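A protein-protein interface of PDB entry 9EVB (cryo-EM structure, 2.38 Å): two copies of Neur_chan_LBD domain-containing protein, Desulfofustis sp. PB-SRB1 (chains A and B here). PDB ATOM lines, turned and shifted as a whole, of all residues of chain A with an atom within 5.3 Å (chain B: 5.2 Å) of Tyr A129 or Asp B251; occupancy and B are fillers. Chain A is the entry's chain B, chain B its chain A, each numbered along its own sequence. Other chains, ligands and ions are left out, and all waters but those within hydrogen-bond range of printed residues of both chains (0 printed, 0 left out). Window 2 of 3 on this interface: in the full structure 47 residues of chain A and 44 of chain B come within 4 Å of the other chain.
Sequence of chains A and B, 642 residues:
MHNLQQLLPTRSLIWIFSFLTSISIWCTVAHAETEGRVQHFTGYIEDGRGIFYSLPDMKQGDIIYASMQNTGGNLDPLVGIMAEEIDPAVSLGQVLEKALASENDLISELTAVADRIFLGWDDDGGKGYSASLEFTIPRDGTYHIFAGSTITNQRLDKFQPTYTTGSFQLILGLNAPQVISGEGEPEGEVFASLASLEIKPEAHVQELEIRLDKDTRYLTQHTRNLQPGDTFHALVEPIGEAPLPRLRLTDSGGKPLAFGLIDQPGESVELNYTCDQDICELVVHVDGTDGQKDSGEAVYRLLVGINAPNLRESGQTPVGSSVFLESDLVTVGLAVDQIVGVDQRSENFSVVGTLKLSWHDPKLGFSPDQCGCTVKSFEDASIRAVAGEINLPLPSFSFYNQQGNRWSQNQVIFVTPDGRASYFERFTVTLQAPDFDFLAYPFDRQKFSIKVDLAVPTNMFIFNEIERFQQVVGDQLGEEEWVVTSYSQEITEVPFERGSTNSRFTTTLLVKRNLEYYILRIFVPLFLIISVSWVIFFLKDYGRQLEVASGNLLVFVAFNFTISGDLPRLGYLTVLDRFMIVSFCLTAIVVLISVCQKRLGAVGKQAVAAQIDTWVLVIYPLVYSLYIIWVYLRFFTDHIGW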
ATOM      1  N   ASP A  76     -21.911  21.667  11.622  1.00  0.00           N
ATOM      2  CA  ASP A  76     -22.111  20.221  11.689  1.00  0.00           C
ATOM      3  C   ASP A  76     -20.771  19.595  12.061  1.00  0.00           C
ATOM      4  O   ASP A  76     -19.818  19.655  11.266  1.00  0.00           O
ATOM      5  CB  ASP A  76     -22.600  19.704  10.339  1.00  0.00           C
ATOM      6  CG  ASP A  76     -23.337  18.407  10.466  1.00  0.00           C
ATOM      7  OD1 ASP A  76     -22.908  17.562  11.278  1.00  0.00           O
ATOM      8  OD2 ASP A  76     -24.344  18.238   9.756  1.00  0.00           O
ATOM      9  N   PRO A  77     -20.627  19.036  13.263  1.00  0.00           N
ATOM     10  CA  PRO A  77     -19.289  18.620  13.706  1.00  0.00           C
ATOM     11  C   PRO A  77     -18.762  17.416  12.941  1.00  0.00           C
ATOM     12  O   PRO A  77     -19.518  16.579  12.445  1.00  0.00           O
ATOM     13  CB  PRO A  77     -19.506  18.278  15.186  1.00  0.00           C
ATOM     14  CG  PRO A  77     -20.740  19.021  15.582  1.00  0.00           C
ATOM     15  CD  PRO A  77     -21.596  19.121  14.368  1.00  0.00           C
ATOM     16  N   ASP A 123     -19.134  11.051  11.913  1.00  0.00           N
ATOM     17  CA  ASP A 123     -19.856  12.231  11.444  1.00  0.00           C
ATOM     18  C   ASP A 123     -21.090  12.513  12.298  1.00  0.00           C
ATOM     19  O   ASP A 123     -21.241  13.607  12.848  1.00  0.00           O
ATOM     20  CB  ASP A 123     -20.249  12.029   9.971  1.00  0.00           C
ATOM     21  CG  ASP A 123     -20.572  13.329   9.262  1.00  0.00           C
ATOM     22  OD1 ASP A 123     -20.934  14.312   9.941  1.00  0.00           O
ATOM     23  OD2 ASP A 123     -20.473  13.359   8.015  1.00  0.00           O
ATOM     24  N   ASP A 124     -21.971  11.523  12.425  1.00  0.00           N
ATOM     25  CA  ASP A 124     -23.253  11.607  13.128  1.00  0.00           C
ATOM     26  C   ASP A 124     -23.386  10.379  14.023  1.00  0.00           C
ATOM     27  O   ASP A 124     -23.720   9.291  13.546  1.00  0.00           O
ATOM     28  CB  ASP A 124     -24.424  11.698  12.152  1.00  0.00           C
ATOM     29  CG  ASP A 124     -24.285  12.844  11.169  1.00  0.00           C
ATOM     30  OD1 ASP A 124     -23.781  13.917  11.563  1.00  0.00           O
ATOM     31  OD2 ASP A 124     -24.680  12.670   9.997  1.00  0.00           O
ATOM     32  N   GLY A 126     -24.264  11.072  17.777  1.00  0.00           N
ATOM     33  CA  GLY A 126     -25.076  11.520  18.886  1.00  0.00           C
ATOM     34  C   GLY A 126     -26.467  11.949  18.458  1.00  0.00           C
ATOM     35  O   GLY A 126     -26.956  11.624  17.379  1.00  0.00           O
ATOM     36  N   LYS A 127     -27.112  12.695  19.350  1.00  0.00           N
ATOM     37  CA  LYS A 127     -28.471  13.167  19.116  1.00  0.00           C
ATOM     38  C   LYS A 127     -28.412  14.296  18.094  1.00  0.00           C
ATOM     39  O   LYS A 127     -27.825  15.353  18.346  1.00  0.00           O
ATOM     40  CB  LYS A 127     -29.117  13.623  20.422  1.00  0.00           C
ATOM     41  CG  LYS A 127     -30.456  14.324  20.246  1.00  0.00           C
ATOM     42  CD  LYS A 127     -30.956  14.916  21.558  1.00  0.00           C
ATOM     43  CE  LYS A 127     -32.233  15.716  21.352  1.00  0.00           C
ATOM     44  NZ  LYS A 127     -32.711  16.326  22.624  1.00  0.00           N
ATOM     45  N   GLY A 128     -28.970  14.049  16.919  1.00  0.00           N
ATOM     46  CA  GLY A 128     -28.922  15.023  15.844  1.00  0.00           C
ATOM     47  C   GLY A 128     -27.662  14.872  15.014  1.00  0.00           C
ATOM     48  O   GLY A 128     -27.309  13.763  14.611  1.00  0.00           O
ATOM     49  N   TYR A 129     -26.989  15.991  14.758  1.00  0.00           N
ATOM     50  CA  TYR A 129     -25.793  16.020  13.929  1.00  0.00           C
ATOM     51  C   TYR A 129     -24.503  16.015  14.747  1.00  0.00           C
ATOM     52  O   TYR A 129     -23.434  16.295  14.195  1.00  0.00           O
ATOM     53  CB  TYR A 129     -25.825  17.241  13.009  1.00  0.00           C
ATOM     54  CG  TYR A 129     -27.041  17.314  12.107  1.00  0.00           C
ATOM     55  CD1 TYR A 129     -27.630  16.157  11.611  1.00  0.00           C
ATOM     56  CD2 TYR A 129     -27.595  18.537  11.751  1.00  0.00           C
ATOM     57  CE1 TYR A 129     -28.743  16.218  10.792  1.00  0.00           C
ATOM     58  CE2 TYR A 129     -28.705  18.606  10.931  1.00  0.00           C
ATOM     59  CZ  TYR A 129     -29.276  17.444  10.455  1.00  0.00           C
ATOM     60  OH  TYR A 129     -30.380  17.508   9.639  1.00  0.00           O
ATOM     61  N   SER A 130     -24.576  15.705  16.038  1.00  0.00           N
ATOM     62  CA  SER A 130     -23.402  15.674  16.896  1.00  0.00           C
ATOM     63  C   SER A 130     -22.624  14.377  16.699  1.00  0.00           C
ATOM     64  O   SER A 130     -23.153  13.374  16.219  1.00  0.00           O
ATOM     65  CB  SER A 130     -23.799  15.818  18.365  1.00  0.00           C
ATOM     66  OG  SER A 130     -24.750  14.837  18.724  1.00  0.00           O
ATOM     67  N   ALA A 131     -21.359  14.395  17.105  1.00  0.00           N
ATOM     68  CA  ALA A 131     -20.465  13.283  16.838  1.00  0.00           C
ATOM     69  C   ALA A 131     -20.076  12.589  18.137  1.00  0.00           C
ATOM     70  O   ALA A 131     -20.063  13.201  19.210  1.00  0.00           O
ATOM     71  CB  ALA A 131     -19.210  13.764  16.105  1.00  0.00           C
ATOM     72  N   SER A 367     -28.836  25.163  13.270  1.00  0.00           N
ATOM     73  CA  SER A 367     -28.677  23.723  13.001  1.00  0.00           C
ATOM     74  C   SER A 367     -30.023  23.047  12.773  1.00  0.00           C
ATOM     75  O   SER A 367     -30.892  23.096  13.656  1.00  0.00           O
ATOM     76  CB  SER A 367     -27.936  23.016  14.136  1.00  0.00           C
ATOM     77  OG  SER A 367     -27.431  21.777  13.662  1.00  0.00           O
ATOM     78  N   PRO A 368     -30.215  22.371  11.635  1.00  0.00           N
ATOM     79  CA  PRO A 368     -31.517  21.755  11.329  1.00  0.00           C
ATOM     80  C   PRO A 368     -32.002  20.736  12.358  1.00  0.00           C
ATOM     81  O   PRO A 368     -33.214  20.680  12.597  1.00  0.00           O
ATOM     82  CB  PRO A 368     -31.282  21.108   9.952  1.00  0.00           C
ATOM     83  CG  PRO A 368     -30.145  21.909   9.345  1.00  0.00           C
ATOM     84  CD  PRO A 368     -29.278  22.289  10.509  1.00  0.00           C
ATOM     85  N   ASP A 369     -31.129  19.906  12.952  1.00  0.00           N
ATOM     86  CA  ASP A 369     -31.613  18.997  13.998  1.00  0.00           C
ATOM     87  C   ASP A 369     -32.241  19.682  15.223  1.00  0.00           C
ATOM     88  O   ASP A 369     -32.848  18.978  16.037  1.00  0.00           O
ATOM     89  CB  ASP A 369     -30.482  18.062  14.446  1.00  0.00           C
ATOM     90  CG  ASP A 369     -29.268  18.815  14.928  1.00  0.00           C
ATOM     91  OD1 ASP A 369     -29.273  20.045  14.785  1.00  0.00           O
ATOM     92  OD2 ASP A 369     -28.307  18.190  15.434  1.00  0.00           O
ATOM     93  N   LEU B 249     -32.549  10.926  -1.990  1.00  0.00           N
ATOM     94  CA  LEU B 249     -33.266  10.759  -0.734  1.00  0.00           C
ATOM     95  C   LEU B 249     -32.529  11.457   0.399  1.00  0.00           C
ATOM     96  O   LEU B 249     -31.330  11.234   0.600  1.00  0.00           O
ATOM     97  CB  LEU B 249     -33.449   9.275  -0.409  1.00  0.00           C
ATOM     98  CG  LEU B 249     -34.335   8.935   0.789  1.00  0.00           C
ATOM     99  CD1 LEU B 249     -35.782   9.362   0.547  1.00  0.00           C
ATOM    100  CD2 LEU B 249     -34.249   7.448   1.093  1.00  0.00           C
ATOM    101  N   THR B 250     -33.261  12.285   1.147  1.00  0.00           N
ATOM    102  CA  THR B 250     -32.718  13.015   2.283  1.00  0.00           C
ATOM    103  C   THR B 250     -33.687  12.928   3.454  1.00  0.00           C
ATOM    104  O   THR B 250     -34.879  12.666   3.284  1.00  0.00           O
ATOM    105  CB  THR B 250     -32.382  14.492   1.979  1.00  0.00           C
ATOM    106  OG1 THR B 250     -33.553  15.200   1.547  1.00  0.00           O
ATOM    107  CG2 THR B 250     -31.281  14.578   0.918  1.00  0.00           C
ATOM    108  N   ASP B 251     -33.159  13.148   4.650  1.00  0.00           N
ATOM    109  CA  ASP B 251     -33.971  13.186   5.859  1.00  0.00           C
ATOM    110  C   ASP B 251     -34.703  14.533   5.951  1.00  0.00           C
ATOM    111  O   ASP B 251     -34.680  15.344   5.021  1.00  0.00           O
ATOM    112  CB  ASP B 251     -33.088  12.911   7.070  1.00  0.00           C
ATOM    113  CG  ASP B 251     -32.254  14.110   7.448  1.00  0.00           C
ATOM    114  OD1 ASP B 251     -31.735  14.819   6.550  1.00  0.00           O
ATOM    115  OD2 ASP B 251     -32.057  14.305   8.662  1.00  0.00           O
ATOM    116  N   SER B 252     -35.364  14.788   7.088  1.00  0.00           N
ATOM    117  CA  SER B 252     -36.114  16.032   7.268  1.00  0.00           C
ATOM    118  C   SER B 252     -35.219  17.261   7.336  1.00  0.00           C
ATOM    119  O   SER B 252     -35.726  18.386   7.286  1.00  0.00           O
ATOM    120  CB  SER B 252     -36.969  15.968   8.530  1.00  0.00           C
ATOM    121  OG  SER B 252     -37.953  14.962   8.421  1.00  0.00           O
ATOM    122  N   GLY B 253     -33.932  17.082   7.616  1.00  0.00           N
ATOM    123  CA  GLY B 253     -33.035  18.213   7.708  1.00  0.00           C
ATOM    124  C   GLY B 253     -32.222  18.434   6.472  1.00  0.00           C
ATOM    125  O   GLY B 253     -31.506  19.433   6.362  1.00  0.00           O
ATOM    126  N   GLY B 254     -32.310  17.498   5.537  1.00  0.00           N
ATOM    127  CA  GLY B 254     -31.584  17.578   4.296  1.00  0.00           C
ATOM    128  C   GLY B 254     -30.340  16.725   4.214  1.00  0.00           C
ATOM    129  O   GLY B 254     -29.639  16.796   3.196  1.00  0.00           O
ATOM    130  N   LYS B 255     -30.033  15.923   5.230  1.00  0.00           N
ATOM    131  CA  LYS B 255     -28.805  15.149   5.138  1.00  0.00           C
ATOM    132  C   LYS B 255     -28.977  14.068   4.085  1.00  0.00           C
ATOM    133  O   LYS B 255     -29.944  13.297   4.154  1.00  0.00           O
ATOM    134  CB  LYS B 255     -28.424  14.541   6.477  1.00  0.00           C
ATOM    135  CG  LYS B 255     -26.944  14.656   6.733  1.00  0.00           C
ATOM    136  CD  LYS B 255     -26.212  13.439   6.223  1.00  0.00           C
ATOM    137  CE  LYS B 255     -24.724  13.576   6.428  1.00  0.00           C
ATOM    138  NZ  LYS B 255     -24.423  13.509   7.875  1.00  0.00           N
ATOM    139  N   PRO B 256     -28.092  13.972   3.099  1.00  0.00           N
ATOM    140  CA  PRO B 256     -28.280  12.961   2.055  1.00  0.00           C
ATOM    141  C   PRO B 256     -28.110  11.547   2.595  1.00  0.00           C
ATOM    142  O   PRO B 256     -27.299  11.293   3.489  1.00  0.00           O
ATOM    143  CB  PRO B 256     -27.193  13.311   1.033  1.00  0.00           C
ATOM    144  CG  PRO B 256     -26.151  14.003   1.845  1.00  0.00           C
ATOM    145  CD  PRO B 256     -26.942  14.843   2.802  1.00  0.00           C
ATOM    146  N   LEU B 257     -28.917  10.628   2.058  1.00  0.00           N
ATOM    147  CA  LEU B 257     -28.930   9.226   2.470  1.00  0.00           C
ATOM    148  C   LEU B 257     -28.756   8.265   1.305  1.00  0.00           C
ATOM    149  O   LEU B 257     -28.097   7.231   1.460  1.00  0.00           O
ATOM    150  CB  LEU B 257     -30.240   8.890   3.217  1.00  0.00           C
ATOM    151  CG  LEU B 257     -30.507   9.668   4.507  1.00  0.00           C
ATOM    152  CD1 LEU B 257     -31.834   9.303   5.178  1.00  0.00           C
ATOM    153  CD2 LEU B 257     -29.347   9.514   5.486  1.00  0.00           C
ATOM    154  N   GLU B 281     -37.423   9.876   9.400  1.00  0.00           N
ATOM    155  CA  GLU B 281     -38.333  10.650   8.567  1.00  0.00           C
ATOM    156  C   GLU B 281     -37.631  10.956   7.249  1.00  0.00           C
ATOM    157  O   GLU B 281     -36.521  11.494   7.248  1.00  0.00           O
ATOM    158  CB  GLU B 281     -38.764  11.930   9.278  1.00  0.00           C
ATOM    159  CG  GLU B 281     -39.289  11.694  10.685  1.00  0.00           C
ATOM    160  CD  GLU B 281     -39.707  12.977  11.370  1.00  0.00           C
ATOM    161  OE1 GLU B 281     -39.416  14.056  10.812  1.00  0.00           O
ATOM    162  OE2 GLU B 281     -40.205  12.910  12.515  1.00  0.00           O
ATOM    163  N   LEU B 282     -38.270  10.612   6.133  1.00  0.00           N
ATOM    164  CA  LEU B 282     -37.619  10.657   4.836  1.00  0.00           C
ATOM    165  C   LEU B 282     -38.297  11.676   3.930  1.00  0.00           C
ATOM    166  O   LEU B 282     -39.507  11.912   4.027  1.00  0.00           O
ATOM    167  CB  LEU B 282     -37.625   9.274   4.171  1.00  0.00           C
ATOM    168  CG  LEU B 282     -37.067   8.091   4.973  1.00  0.00           C
ATOM    169  CD1 LEU B 282     -37.001   6.859   4.109  1.00  0.00           C
ATOM    170  CD2 LEU B 282     -35.680   8.391   5.492  1.00  0.00           C
ATOM    171  N   VAL B 283     -37.502  12.276   3.043  1.00  0.00           N
ATOM    172  CA  VAL B 283     -37.987  13.227   2.049  1.00  0.00           C
ATOM    173  C   VAL B 283     -37.426  12.845   0.689  1.00  0.00           C
ATOM    174  O   VAL B 283     -36.217  12.622   0.550  1.00  0.00           O
ATOM    175  CB  VAL B 283     -37.591  14.679   2.385  1.00  0.00           C
ATOM    176  CG1 VAL B 283     -38.167  15.633   1.343  1.00  0.00           C
ATOM    177  CG2 VAL B 283     -38.054  15.055   3.778  1.00  0.00           C
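The side-chain amino group of Lys B255 lies within salt-bridge range of the side-chain carboxylate of Asp A123, 3.96 Å away. The side-chain amino group of Lys B255 is in salt-bridge range of the side-chain carboxylate of Asp A124 (3.8 Å).
OD1 of Asp B251 lies close to N of Gly B253, at 3.3 Å. OD1 of Asp B251 lies within hydrogen-bond range of N of Gly B254 (2.9 Å). The side-chain carboxylate (OD1) of Asp B251 is in hydrogen-bond range of the backbone NH (N) of Lys B255 (2.4 Å). The side-chain carboxylate (OD2) of Asp A369 is in hydrogen-bond range of the backbone NH (N) of Tyr A129, 2.7 Å away.
Among the printed residues, merely in contact across the chains: Tyr A129 with Gly B253 (3.4 Å), Tyr A129 with Asp B251 (3.7 Å) and Pro A368 with Gly B253 (3.97 Å).
Of chain B, only Asp B251 (3.7 Å) and Gly B253 (3.4 Å) come within 4 Å of Tyr A129. Of the printed residues of chain B, Asp A123 touches Lys B255. Printed residues of chain A within 4 Å of Lys B255: Asp A123 (3.96 Å) and Asp A124 (2.3 Å). Printed residues of chain B within 4 Å of Asp A124: Lys B255. Of the printed residues of chain A, Gly B253 touches Tyr A129 (3.4 Å) and Pro A368 (3.97 Å). Ser B252 touches none of the printed residues of chain A. Lys A127 touches none of the printed residues of chain B.
Of the 13 printed residues of chain A, 4 touch a printed residue of chain B. Hydrophobic or aromatic side chains of chain A that line the printed part of chain B: Tyr A129 and Pro A368. Of the 12 printed residues of chain B, 3 touch a printed residue of chain A. Printed residues of chain B that touch a printed residue of chain A: Asp B251, Gly B253 and Lys B255. Among the printed residues, Asp or Glu carboxylates within 4 Å of a Lys or Arg side-chain nitrogen of the other chain: Asp A123 with Lys B255 (3.96 Å) and Asp A124 with Lys B255 (2.3 Å).
No position is printed for both chains.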
